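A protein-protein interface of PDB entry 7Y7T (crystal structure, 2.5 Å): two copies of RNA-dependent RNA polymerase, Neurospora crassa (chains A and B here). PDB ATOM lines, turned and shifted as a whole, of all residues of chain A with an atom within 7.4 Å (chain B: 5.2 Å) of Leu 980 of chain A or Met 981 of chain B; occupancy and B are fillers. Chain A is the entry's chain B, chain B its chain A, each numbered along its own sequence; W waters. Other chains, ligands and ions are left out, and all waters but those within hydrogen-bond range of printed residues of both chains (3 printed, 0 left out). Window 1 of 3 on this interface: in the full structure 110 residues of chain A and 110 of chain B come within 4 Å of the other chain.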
ATOM      1  N   ARG A 466      -4.333  17.192  -8.779  1.00  0.00           N
ATOM      2  CA  ARG A 466      -5.517  16.435  -8.386  1.00  0.00           C
ATOM      3  C   ARG A 466      -6.163  17.025  -7.141  1.00  0.00           C
ATOM      4  O   ARG A 466      -7.395  17.113  -7.059  1.00  0.00           O
ATOM      5  CB  ARG A 466      -5.171  14.965  -8.168  1.00  0.00           C
ATOM      6  CG  ARG A 466      -6.406  14.087  -8.052  1.00  0.00           C
ATOM      7  CD  ARG A 466      -6.048  12.628  -7.850  1.00  0.00           C
ATOM      8  NE  ARG A 466      -5.190  12.429  -6.690  1.00  0.00           N
ATOM      9  CZ  ARG A 466      -4.613  11.277  -6.377  1.00  0.00           C
ATOM     10  NH1 ARG A 466      -4.789  10.192  -7.115  1.00  0.00           N
ATOM     11  NH2 ARG A 466      -3.836  11.213  -5.300  1.00  0.00           N
ATOM     12  N   GLN A 467      -5.353  17.426  -6.157  1.00  0.00           N
ATOM     13  CA  GLN A 467      -5.872  18.201  -5.034  1.00  0.00           C
ATOM     14  C   GLN A 467      -6.650  19.406  -5.527  1.00  0.00           C
ATOM     15  O   GLN A 467      -7.824  19.594  -5.190  1.00  0.00           O
ATOM     16  CB  GLN A 467      -4.730  18.670  -4.134  1.00  0.00           C
ATOM     17  CG  GLN A 467      -4.059  17.581  -3.362  1.00  0.00           C
ATOM     18  CD  GLN A 467      -4.905  17.054  -2.222  1.00  0.00           C
ATOM     19  OE1 GLN A 467      -4.566  16.042  -1.618  1.00  0.00           O
ATOM     20  NE2 GLN A 467      -6.000  17.744  -1.910  1.00  0.00           N
ATOM     21  N   TYR A 470      -9.852  18.746  -7.151  1.00  0.00           N
ATOM     22  CA  TYR A 470     -10.818  18.301  -6.152  1.00  0.00           C
ATOM     23  C   TYR A 470     -11.267  19.454  -5.263  1.00  0.00           C
ATOM     24  O   TYR A 470     -12.458  19.582  -4.961  1.00  0.00           O
ATOM     25  CB  TYR A 470     -10.247  17.179  -5.288  1.00  0.00           C
ATOM     26  CG  TYR A 470     -11.150  16.912  -4.111  1.00  0.00           C
ATOM     27  CD1 TYR A 470     -12.405  16.358  -4.305  1.00  0.00           C
ATOM     28  CD2 TYR A 470     -10.775  17.255  -2.819  1.00  0.00           C
ATOM     29  CE1 TYR A 470     -13.254  16.131  -3.251  1.00  0.00           C
ATOM     30  CE2 TYR A 470     -11.624  17.029  -1.750  1.00  0.00           C
ATOM     31  CZ  TYR A 470     -12.864  16.465  -1.978  1.00  0.00           C
ATOM     32  OH  TYR A 470     -13.734  16.230  -0.942  1.00  0.00           O
ATOM     33  N   ARG A 479     -22.027  12.070  -6.749  1.00  0.00           N
ATOM     34  CA  ARG A 479     -21.515  10.718  -6.561  1.00  0.00           C
ATOM     35  C   ARG A 479     -22.424   9.903  -5.649  1.00  0.00           C
ATOM     36  O   ARG A 479     -22.629   8.706  -5.880  1.00  0.00           O
ATOM     37  CB  ARG A 479     -20.094  10.770  -5.999  1.00  0.00           C
ATOM     38  CG  ARG A 479     -19.050  11.242  -6.998  1.00  0.00           C
ATOM     39  CD  ARG A 479     -17.753  11.613  -6.299  1.00  0.00           C
ATOM     40  NE  ARG A 479     -16.610  11.564  -7.201  1.00  0.00           N
ATOM     41  CZ  ARG A 479     -15.419  11.083  -6.873  1.00  0.00           C
ATOM     42  NH1 ARG A 479     -15.183  10.576  -5.674  1.00  0.00           N
ATOM     43  NH2 ARG A 479     -14.439  11.108  -7.773  1.00  0.00           N
ATOM     44  N   GLU A 497     -14.186  15.729 -13.028  1.00  0.00           N
ATOM     45  CA  GLU A 497     -14.021  14.289 -12.860  1.00  0.00           C
ATOM     46  C   GLU A 497     -13.243  13.673 -14.015  1.00  0.00           C
ATOM     47  O   GLU A 497     -12.525  12.687 -13.819  1.00  0.00           O
ATOM     48  CB  GLU A 497     -15.386  13.616 -12.715  1.00  0.00           C
ATOM     49  CG  GLU A 497     -16.160  14.042 -11.476  1.00  0.00           C
ATOM     50  CD  GLU A 497     -15.798  13.224 -10.251  1.00  0.00           C
ATOM     51  OE1 GLU A 497     -14.591  13.045  -9.980  1.00  0.00           O
ATOM     52  OE2 GLU A 497     -16.724  12.765  -9.551  1.00  0.00           O
ATOM     53  N   MET A 972     -10.378  -0.301  -9.542  1.00  0.00           N
ATOM     54  CA  MET A 972     -11.512   0.034  -8.696  1.00  0.00           C
ATOM     55  C   MET A 972     -12.824  -0.211  -9.432  1.00  0.00           C
ATOM     56  O   MET A 972     -12.913  -0.053 -10.650  1.00  0.00           O
ATOM     57  CB  MET A 972     -11.452   1.501  -8.271  1.00  0.00           C
ATOM     58  CG  MET A 972     -10.082   2.007  -7.862  1.00  0.00           C
ATOM     59  SD  MET A 972      -9.729   1.636  -6.139  1.00  0.00           S
ATOM     60  CE  MET A 972     -11.031   2.585  -5.358  1.00  0.00           C
ATOM     61  N   PHE A 975     -18.403   2.124  -8.061  1.00  0.00           N
ATOM     62  CA  PHE A 975     -18.893   2.592  -6.769  1.00  0.00           C
ATOM     63  C   PHE A 975     -17.743   2.906  -5.818  1.00  0.00           C
ATOM     64  O   PHE A 975     -17.676   4.004  -5.255  1.00  0.00           O
ATOM     65  CB  PHE A 975     -19.828   1.555  -6.150  1.00  0.00           C
ATOM     66  CG  PHE A 975     -20.149   1.821  -4.711  1.00  0.00           C
ATOM     67  CD1 PHE A 975     -20.957   2.890  -4.358  1.00  0.00           C
ATOM     68  CD2 PHE A 975     -19.639   1.013  -3.710  1.00  0.00           C
ATOM     69  CE1 PHE A 975     -21.254   3.144  -3.036  1.00  0.00           C
ATOM     70  CE2 PHE A 975     -19.931   1.262  -2.383  1.00  0.00           C
ATOM     71  CZ  PHE A 975     -20.741   2.329  -2.046  1.00  0.00           C
ATOM     72  N   MET A 976     -16.832   1.948  -5.616  1.00  0.00           N
ATOM     73  CA  MET A 976     -15.722   2.172  -4.693  1.00  0.00           C
ATOM     74  C   MET A 976     -14.847   3.337  -5.136  1.00  0.00           C
ATOM     75  O   MET A 976     -14.268   4.032  -4.292  1.00  0.00           O
ATOM     76  CB  MET A 976     -14.884   0.902  -4.548  1.00  0.00           C
ATOM     77  CG  MET A 976     -15.621  -0.266  -3.909  1.00  0.00           C
ATOM     78  SD  MET A 976     -16.496   0.193  -2.401  1.00  0.00           S
ATOM     79  CE  MET A 976     -15.308  -0.287  -1.148  1.00  0.00           C
ATOM     80  N   TYR A 977     -14.731   3.561  -6.446  1.00  0.00           N
ATOM     81  CA  TYR A 977     -13.999   4.723  -6.940  1.00  0.00           C
ATOM     82  C   TYR A 977     -14.619   6.016  -6.425  1.00  0.00           C
ATOM     83  O   TYR A 977     -13.919   6.886  -5.892  1.00  0.00           O
ATOM     84  CB  TYR A 977     -13.973   4.714  -8.469  1.00  0.00           C
ATOM     85  CG  TYR A 977     -13.218   5.876  -9.078  1.00  0.00           C
ATOM     86  CD1 TYR A 977     -11.848   6.014  -8.893  1.00  0.00           C
ATOM     87  CD2 TYR A 977     -13.878   6.841  -9.834  1.00  0.00           C
ATOM     88  CE1 TYR A 977     -11.152   7.076  -9.445  1.00  0.00           C
ATOM     89  CE2 TYR A 977     -13.189   7.908 -10.391  1.00  0.00           C
ATOM     90  CZ  TYR A 977     -11.828   8.019 -10.193  1.00  0.00           C
ATOM     91  OH  TYR A 977     -11.141   9.077 -10.744  1.00  0.00           O
ATOM     92  N   ALA A 978     -15.940   6.148  -6.559  1.00  0.00           N
ATOM     93  CA  ALA A 978     -16.633   7.378  -6.196  1.00  0.00           C
ATOM     94  C   ALA A 978     -16.574   7.687  -4.707  1.00  0.00           C
ATOM     95  O   ALA A 978     -16.896   8.813  -4.315  1.00  0.00           O
ATOM     96  CB  ALA A 978     -18.094   7.304  -6.645  1.00  0.00           C
ATOM     97  N   GLY A 979     -16.180   6.730  -3.874  1.00  0.00           N
ATOM     98  CA  GLY A 979     -16.081   6.940  -2.446  1.00  0.00           C
ATOM     99  C   GLY A 979     -14.722   7.377  -1.952  1.00  0.00           C
ATOM    100  O   GLY A 979     -14.526   7.497  -0.739  1.00  0.00           O
ATOM    101  N   LEU A 980     -13.774   7.620  -2.853  1.00  0.00           N
ATOM    102  CA  LEU A 980     -12.422   8.015  -2.490  1.00  0.00           C
ATOM    103  C   LEU A 980     -12.203   9.491  -2.797  1.00  0.00           C
ATOM    104  O   LEU A 980     -12.867  10.076  -3.656  1.00  0.00           O
ATOM    105  CB  LEU A 980     -11.383   7.167  -3.232  1.00  0.00           C
ATOM    106  CG  LEU A 980     -11.214   5.705  -2.807  1.00  0.00           C
ATOM    107  CD1 LEU A 980      -9.872   5.181  -3.284  1.00  0.00           C
ATOM    108  CD2 LEU A 980     -11.354   5.532  -1.304  1.00  0.00           C
ATOM    109  N   MET A 981     -11.253  10.082  -2.085  1.00  0.00           N
ATOM    110  CA  MET A 981     -10.914  11.491  -2.199  1.00  0.00           C
ATOM    111  C   MET A 981      -9.406  11.644  -2.094  1.00  0.00           C
ATOM    112  O   MET A 981      -8.725  10.767  -1.551  1.00  0.00           O
ATOM    113  CB  MET A 981     -11.600  12.320  -1.104  1.00  0.00           C
ATOM    114  CG  MET A 981     -11.177  11.920   0.299  1.00  0.00           C
ATOM    115  SD  MET A 981     -11.949  12.881   1.611  1.00  0.00           S
ATOM    116  CE  MET A 981     -12.070  14.477   0.823  1.00  0.00           C
ATOM    117  N   PRO A 982      -8.850  12.745  -2.604  1.00  0.00           N
ATOM    118  CA  PRO A 982      -7.399  12.954  -2.496  1.00  0.00           C
ATOM    119  C   PRO A 982      -6.977  13.218  -1.056  1.00  0.00           C
ATOM    120  O   PRO A 982      -7.576  14.037  -0.356  1.00  0.00           O
ATOM    121  CB  PRO A 982      -7.143  14.173  -3.394  1.00  0.00           C
ATOM    122  CG  PRO A 982      -8.351  14.268  -4.270  1.00  0.00           C
ATOM    123  CD  PRO A 982      -9.486  13.787  -3.427  1.00  0.00           C
ATOM    124  N   ASP A 983      -5.939  12.506  -0.619  1.00  0.00           N
ATOM    125  CA  ASP A 983      -5.349  12.681   0.709  1.00  0.00           C
ATOM    126  C   ASP A 983      -4.505  13.949   0.719  1.00  0.00           C
ATOM    127  O   ASP A 983      -3.376  13.970   0.219  1.00  0.00           O
ATOM    128  CB  ASP A 983      -4.541  11.441   1.084  1.00  0.00           C
ATOM    129  CG  ASP A 983      -3.906  11.521   2.472  1.00  0.00           C
ATOM    130  OD1 ASP A 983      -3.987  12.573   3.143  1.00  0.00           O
ATOM    131  OD2 ASP A 983      -3.344  10.493   2.911  1.00  0.00           O
ATOM    132  N   LYS A 984      -5.059  15.015   1.306  1.00  0.00           N
ATOM    133  CA  LYS A 984      -4.347  16.288   1.367  1.00  0.00           C
ATOM    134  C   LYS A 984      -3.010  16.139   2.074  1.00  0.00           C
ATOM    135  O   LYS A 984      -2.008  16.731   1.656  1.00  0.00           O
ATOM    136  CB  LYS A 984      -5.205  17.344   2.061  1.00  0.00           C
ATOM    137  CG  LYS A 984      -4.546  18.714   2.121  1.00  0.00           C
ATOM    138  CD  LYS A 984      -4.850  19.529   0.878  1.00  0.00           C
ATOM    139  CE  LYS A 984      -4.465  20.989   1.063  1.00  0.00           C
ATOM    140  NZ  LYS A 984      -4.345  21.690  -0.248  1.00  0.00           N
ATOM    141  N   LYS A 985      -2.968  15.344   3.143  1.00  0.00           N
ATOM    142  CA  LYS A 985      -1.715  15.154   3.858  1.00  0.00           C
ATOM    143  C   LYS A 985      -0.727  14.321   3.052  1.00  0.00           C
ATOM    144  O   LYS A 985       0.486  14.471   3.226  1.00  0.00           O
ATOM    145  CB  LYS A 985      -1.980  14.521   5.223  1.00  0.00           C
ATOM    146  CG  LYS A 985      -2.502  15.509   6.253  1.00  0.00           C
ATOM    147  CD  LYS A 985      -2.849  14.829   7.566  1.00  0.00           C
ATOM    148  CE  LYS A 985      -3.663  15.750   8.462  1.00  0.00           C
ATOM    149  NZ  LYS A 985      -4.040  15.092   9.743  1.00  0.00           N
ATOM    150  N   PHE A 986      -1.215  13.451   2.163  1.00  0.00           N
ATOM    151  CA  PHE A 986      -0.308  12.720   1.282  1.00  0.00           C
ATOM    152  C   PHE A 986       0.357  13.661   0.287  1.00  0.00           C
ATOM    153  O   PHE A 986       1.574  13.600   0.076  1.00  0.00           O
ATOM    154  CB  PHE A 986      -1.057  11.609   0.546  1.00  0.00           C
ATOM    155  CG  PHE A 986      -0.186  10.790  -0.371  1.00  0.00           C
ATOM    156  CD1 PHE A 986       0.534   9.711   0.116  1.00  0.00           C
ATOM    157  CD2 PHE A 986      -0.086  11.102  -1.718  1.00  0.00           C
ATOM    158  CE1 PHE A 986       1.335   8.956  -0.723  1.00  0.00           C
ATOM    159  CE2 PHE A 986       0.711  10.351  -2.562  1.00  0.00           C
ATOM    160  CZ  PHE A 986       1.424   9.277  -2.064  1.00  0.00           C
ATOM    161  N   ARG B 466     -14.469  -0.381   4.724  1.00  0.00           N
ATOM    162  CA  ARG B 466     -13.308   0.344   4.214  1.00  0.00           C
ATOM    163  C   ARG B 466     -13.050   1.595   5.042  1.00  0.00           C
ATOM    164  O   ARG B 466     -11.906   1.894   5.402  1.00  0.00           O
ATOM    165  CB  ARG B 466     -13.506   0.707   2.741  1.00  0.00           C
ATOM    166  CG  ARG B 466     -12.341   1.492   2.157  1.00  0.00           C
ATOM    167  CD  ARG B 466     -12.604   1.953   0.731  1.00  0.00           C
ATOM    168  NE  ARG B 466     -13.790   2.797   0.625  1.00  0.00           N
ATOM    169  CZ  ARG B 466     -14.285   3.253  -0.516  1.00  0.00           C
ATOM    170  NH1 ARG B 466     -13.704   2.995  -1.676  1.00  0.00           N
ATOM    171  NH2 ARG B 466     -15.388   3.998  -0.494  1.00  0.00           N
ATOM    172  N   TYR B 470      -9.631   1.997   7.268  1.00  0.00           N
ATOM    173  CA  TYR B 470      -8.821   3.198   7.102  1.00  0.00           C
ATOM    174  C   TYR B 470      -8.636   3.930   8.423  1.00  0.00           C
ATOM    175  O   TYR B 470      -7.559   4.474   8.693  1.00  0.00           O
ATOM    176  CB  TYR B 470      -9.464   4.123   6.069  1.00  0.00           C
ATOM    177  CG  TYR B 470      -8.703   5.408   5.860  1.00  0.00           C
ATOM    178  CD1 TYR B 470      -7.562   5.441   5.071  1.00  0.00           C
ATOM    179  CD2 TYR B 470      -9.118   6.588   6.464  1.00  0.00           C
ATOM    180  CE1 TYR B 470      -6.861   6.618   4.880  1.00  0.00           C
ATOM    181  CE2 TYR B 470      -8.422   7.769   6.283  1.00  0.00           C
ATOM    182  CZ  TYR B 470      -7.293   7.778   5.488  1.00  0.00           C
ATOM    183  OH  TYR B 470      -6.587   8.945   5.294  1.00  0.00           O
ATOM    184  N   ARG B 476      -0.143   6.339   5.933  1.00  0.00           N
ATOM    185  CA  ARG B 476       0.310   7.421   5.064  1.00  0.00           C
ATOM    186  C   ARG B 476       1.830   7.476   4.980  1.00  0.00           C
ATOM    187  O   ARG B 476       2.386   7.761   3.913  1.00  0.00           O
ATOM    188  CB  ARG B 476      -0.245   8.751   5.568  1.00  0.00           C
ATOM    189  CG  ARG B 476      -0.123   9.902   4.590  1.00  0.00           C
ATOM    190  CD  ARG B 476      -0.644  11.171   5.229  1.00  0.00           C
ATOM    191  NE  ARG B 476      -2.100  11.196   5.265  1.00  0.00           N
ATOM    192  CZ  ARG B 476      -2.820  11.202   6.378  1.00  0.00           C
ATOM    193  NH1 ARG B 476      -4.141  11.260   6.347  1.00  0.00           N
ATOM    194  NH2 ARG B 476      -2.199  11.138   7.552  1.00  0.00           N
ATOM    195  N   ASN B 504     -11.934  -2.600  -2.656  1.00  0.00           N
ATOM    196  CA  ASN B 504     -12.020  -1.627  -3.735  1.00  0.00           C
ATOM    197  C   ASN B 504     -12.197  -2.273  -5.102  1.00  0.00           C
ATOM    198  O   ASN B 504     -12.561  -1.573  -6.053  1.00  0.00           O
ATOM    199  CB  ASN B 504     -10.782  -0.731  -3.740  1.00  0.00           C
ATOM    200  CG  ASN B 504     -10.798   0.288  -2.618  1.00  0.00           C
ATOM    201  OD1 ASN B 504     -11.859   0.757  -2.209  1.00  0.00           O
ATOM    202  ND2 ASN B 504      -9.619   0.650  -2.127  1.00  0.00           N
ATOM    203  N   TYR B 977      -3.016   5.637  -6.587  1.00  0.00           N
ATOM    204  CA  TYR B 977      -3.846   4.919  -5.624  1.00  0.00           C
ATOM    205  C   TYR B 977      -3.432   5.237  -4.194  1.00  0.00           C
ATOM    206  O   TYR B 977      -4.284   5.371  -3.308  1.00  0.00           O
ATOM    207  CB  TYR B 977      -3.771   3.415  -5.894  1.00  0.00           C
ATOM    208  CG  TYR B 977      -4.548   2.545  -4.924  1.00  0.00           C
ATOM    209  CD1 TYR B 977      -5.931   2.442  -5.003  1.00  0.00           C
ATOM    210  CD2 TYR B 977      -3.892   1.808  -3.946  1.00  0.00           C
ATOM    211  CE1 TYR B 977      -6.641   1.640  -4.125  1.00  0.00           C
ATOM    212  CE2 TYR B 977      -4.591   1.005  -3.064  1.00  0.00           C
ATOM    213  CZ  TYR B 977      -5.964   0.922  -3.157  1.00  0.00           C
ATOM    214  OH  TYR B 977      -6.659   0.122  -2.279  1.00  0.00           O
ATOM    215  N   GLY B 979      -2.483   7.941  -3.023  1.00  0.00           N
ATOM    216  CA  GLY B 979      -2.809   9.303  -2.652  1.00  0.00           C
ATOM    217  C   GLY B 979      -4.281   9.534  -2.389  1.00  0.00           C
ATOM    218  O   GLY B 979      -4.673  10.616  -1.943  1.00  0.00           O
ATOM    219  N   LEU B 980      -5.107   8.533  -2.666  1.00  0.00           N
ATOM    220  CA  LEU B 980      -6.527   8.631  -2.374  1.00  0.00           C
ATOM    221  C   LEU B 980      -6.822   8.045  -0.997  1.00  0.00           C
ATOM    222  O   LEU B 980      -6.070   7.224  -0.469  1.00  0.00           O
ATOM    223  CB  LEU B 980      -7.355   7.920  -3.447  1.00  0.00           C
ATOM    224  CG  LEU B 980      -7.349   8.579  -4.830  1.00  0.00           C
ATOM    225  CD1 LEU B 980      -8.414   7.971  -5.728  1.00  0.00           C
ATOM    226  CD2 LEU B 980      -7.535  10.084  -4.721  1.00  0.00           C
ATOM    227  N   MET B 981      -7.924   8.498  -0.410  1.00  0.00           N
ATOM    228  CA  MET B 981      -8.362   8.026   0.895  1.00  0.00           C
ATOM    229  C   MET B 981      -9.883   8.018   0.912  1.00  0.00           C
ATOM    230  O   MET B 981     -10.518   8.726   0.122  1.00  0.00           O
ATOM    231  CB  MET B 981      -7.823   8.904   2.035  1.00  0.00           C
ATOM    232  CG  MET B 981      -8.242  10.361   1.951  1.00  0.00           C
ATOM    233  SD  MET B 981      -8.452  11.108   3.585  1.00  0.00           S
ATOM    234  CE  MET B 981      -6.895  11.912   3.901  1.00  0.00           C
ATOM    235  N   PRO B 982     -10.499   7.224   1.792  1.00  0.00           N
ATOM    236  CA  PRO B 982     -11.966   7.172   1.829  1.00  0.00           C
ATOM    237  C   PRO B 982     -12.568   8.457   2.375  1.00  0.00           C
ATOM    238  O   PRO B 982     -12.056   9.053   3.327  1.00  0.00           O
ATOM    239  CB  PRO B 982     -12.260   5.980   2.751  1.00  0.00           C
ATOM    240  CG  PRO B 982     -10.982   5.197   2.800  1.00  0.00           C
ATOM    241  CD  PRO B 982      -9.899   6.220   2.685  1.00  0.00           C
ATOM    242  N   ASP B 983     -13.675   8.873   1.765  1.00  0.00           N
ATOM    243  CA  ASP B 983     -14.360  10.112   2.121  1.00  0.00           C
ATOM    244  C   ASP B 983     -15.469   9.792   3.119  1.00  0.00           C
ATOM    245  O   ASP B 983     -16.502   9.226   2.747  1.00  0.00           O
ATOM    246  CB  ASP B 983     -14.917  10.787   0.870  1.00  0.00           C
ATOM    247  CG  ASP B 983     -15.690  12.057   1.177  1.00  0.00           C
ATOM    248  OD1 ASP B 983     -15.557  12.591   2.298  1.00  0.00           O
ATOM    249  OD2 ASP B 983     -16.437  12.520   0.292  1.00  0.00           O
HETATM  250  O   HOH W   1     -17.635   3.561  -2.584  1.00  0.00           O
HETATM  251  O   HOH W   2      -1.006  10.016  -5.174  1.00  0.00           O
HETATM  252  O   HOH W   3     -16.255   6.082   0.844  1.00  0.00           O
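N of Asp 983 of chain B sits at hydrogen-bond distance from O of Gly 979 of chain A, at 3.0 Å. N of Met 981 of chain B sits at hydrogen-bond distance from O of Met 981 of chain A, at 2.7 Å. The backbone carbonyl oxygen (O) of Gly 979 of chain B is in hydrogen-bond range of the backbone NH (N) of Asp 983 of chain A (2.6 Å). OD1 of Asp 983 of chain B sits close to SD of Met 981 of chain A (3.7 Å). The guanidinium group (NH1) of Arg 466 of chain B is in hydrogen-bond range of the backbone carbonyl oxygen (O) of Met 976 of chain A. NE of Arg 476 of chain B is in salt-bridge range of OD2 of Asp 983 of chain A (2.8 Å).
Water W3 bridges NH2 of Arg 466 of chain B (2.6 Å) and O of Gly 979 of chain A (2.7 Å). Water W1 lies within hydrogen-bond range of the backbone carbonyl oxygen (O) of Phe 975 of chain A (2.7 Å), the guanidinium group (NH2) of Arg 466 of chain B (3.1 Å) and the side-chain sulfur (SD) of Met 976 of chain A (3.6 Å). Water W2 lies within hydrogen-bond range of NH2 of Arg 466 of chain A (3.1 Å) and N of Gly 979 of chain B (3.3 Å).
The side-chain hydroxyl (OH) of Tyr 977 of chain B is in hydrogen-bond range of the side-chain amide nitrogen (ND2) of Asn 504 of chain B (3.0 Å). The guanidinium group (NH1) of Arg 466 of chain B lies within hydrogen-bond range of the side-chain amide oxygen (OD1) of Asn 504 of chain B (2.9 Å). OH of Tyr 470 of chain B sits close to SD of Met 981 of chain B (3.3 Å). The side-chain carboxylate (OD1) of Asp 983 of chain A sits at hydrogen-bond distance from the backbone NH (N) of Lys 985 of chain A, 3.0 Å away. The guanidinium group of Arg 479 of chain A is in hydrogen-bond range of the backbone carbonyl oxygen of Leu 980 of chain A, at 3.1 Å. OD1 of Asp 983 of chain A sits at hydrogen-bond distance from N of Phe 986 of chain A (3.1 Å).
Of the 10 printed residues of chain B, 9 touch a printed residue of chain A. Hydrophobic or aromatic side chains of chain B that line the printed part of chain A: Tyr 977, Leu 980 and Met 981. Among the printed residues, Asp or Glu carboxylates within 4 Å of a Lys or Arg side-chain nitrogen of the other chain: Asp 983 of chain A with Arg 476 of chain B.
Arg 466 of chain A touches Gly 979 of chain B, and with the chains exchanged Gly 979 of chain A touches Arg 466 of chain B. Leu 980 of chain B touches its own counterpart, Leu 980 of chain A. Met 981 of chain A touches its own counterpart, Met 981 of chain B. Met 981 of chain A touches Asp 983 of chain B, and with the chains exchanged Asp 983 of chain A touches Met 981 of chain B. Of the 24 pairs that touch across the chains among the printed residues, 16 have their exchanged pair printed and touching as well.
Glu 497 of chain A touches none of the printed residues of chain B. Leu 980 of chain A touches just these residues of chain B: Arg 466 (3.5 Å), Leu 980 (3.7 Å), Met 981 (3.3 Å) and Pro 982 (3.6 Å). Printed residues of chain B within 4 Å of Pro 982 of chain A: Gly 979 (3.6 Å) and Leu 980 (3.6 Å). Printed residues of chain B within 4 Å of Asp 983 of chain A: Arg 476 (2.8 Å), Gly 979 (2.6 Å) and Met 981 (3.1 Å). Of the printed residues of chain A, Asn 504 of chain B touches Met 972 and Met 976. Met 981 of chain B touches just these residues of chain A: Leu 980 (3.3 Å), Met 981 (2.7 Å) and Asp 983 (3.1 Å). The nearest residue of chain A that does not touch Met 981 of chain B is Gly 979 of chain A (4.3 Å).
Among the printed residues, pairs that only touch across the chains: Arg 466 of chain A with Gly 979 of chain B (3.4 Å), Arg 466 of chain A with Leu 980 of chain B (3.6 Å), Met 972 of chain A with Asn 504 of chain B (3.3 Å), Met 972 of chain A with Tyr 977 of chain B (3.7 Å), Met 976 of chain A with Asn 504 of chain B (3.7 Å), Gly 979 of chain A with Arg 466 of chain B (3.6 Å), Gly 979 of chain A with Pro 982 of chain B (3.6 Å), Leu 980 of chain A with Arg 466 of chain B (3.5 Å), Leu 980 of chain A with Leu 980 of chain B (3.7 Å), Leu 980 of chain A with Met 981 of chain B (3.3 Å), Leu 980 of chain A with Pro 982 of chain B (3.6 Å), Met 981 of chain A with Leu 980 of chain B (3.2 Å), Pro 982 of chain A with Gly 979 of chain B (3.6 Å), Pro 982 of chain A with Leu 980 of chain B (3.6 Å), Asp 983 of chain A with Met 981 of chain B (3.1 Å), Lys 985 of chain A with Arg 476 of chain B (3.3 Å), Phe 986 of chain A with Arg 476 of chain B (3.9 Å) and Phe 986 of chain A with Gly 979 of chain B (3.4 Å).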
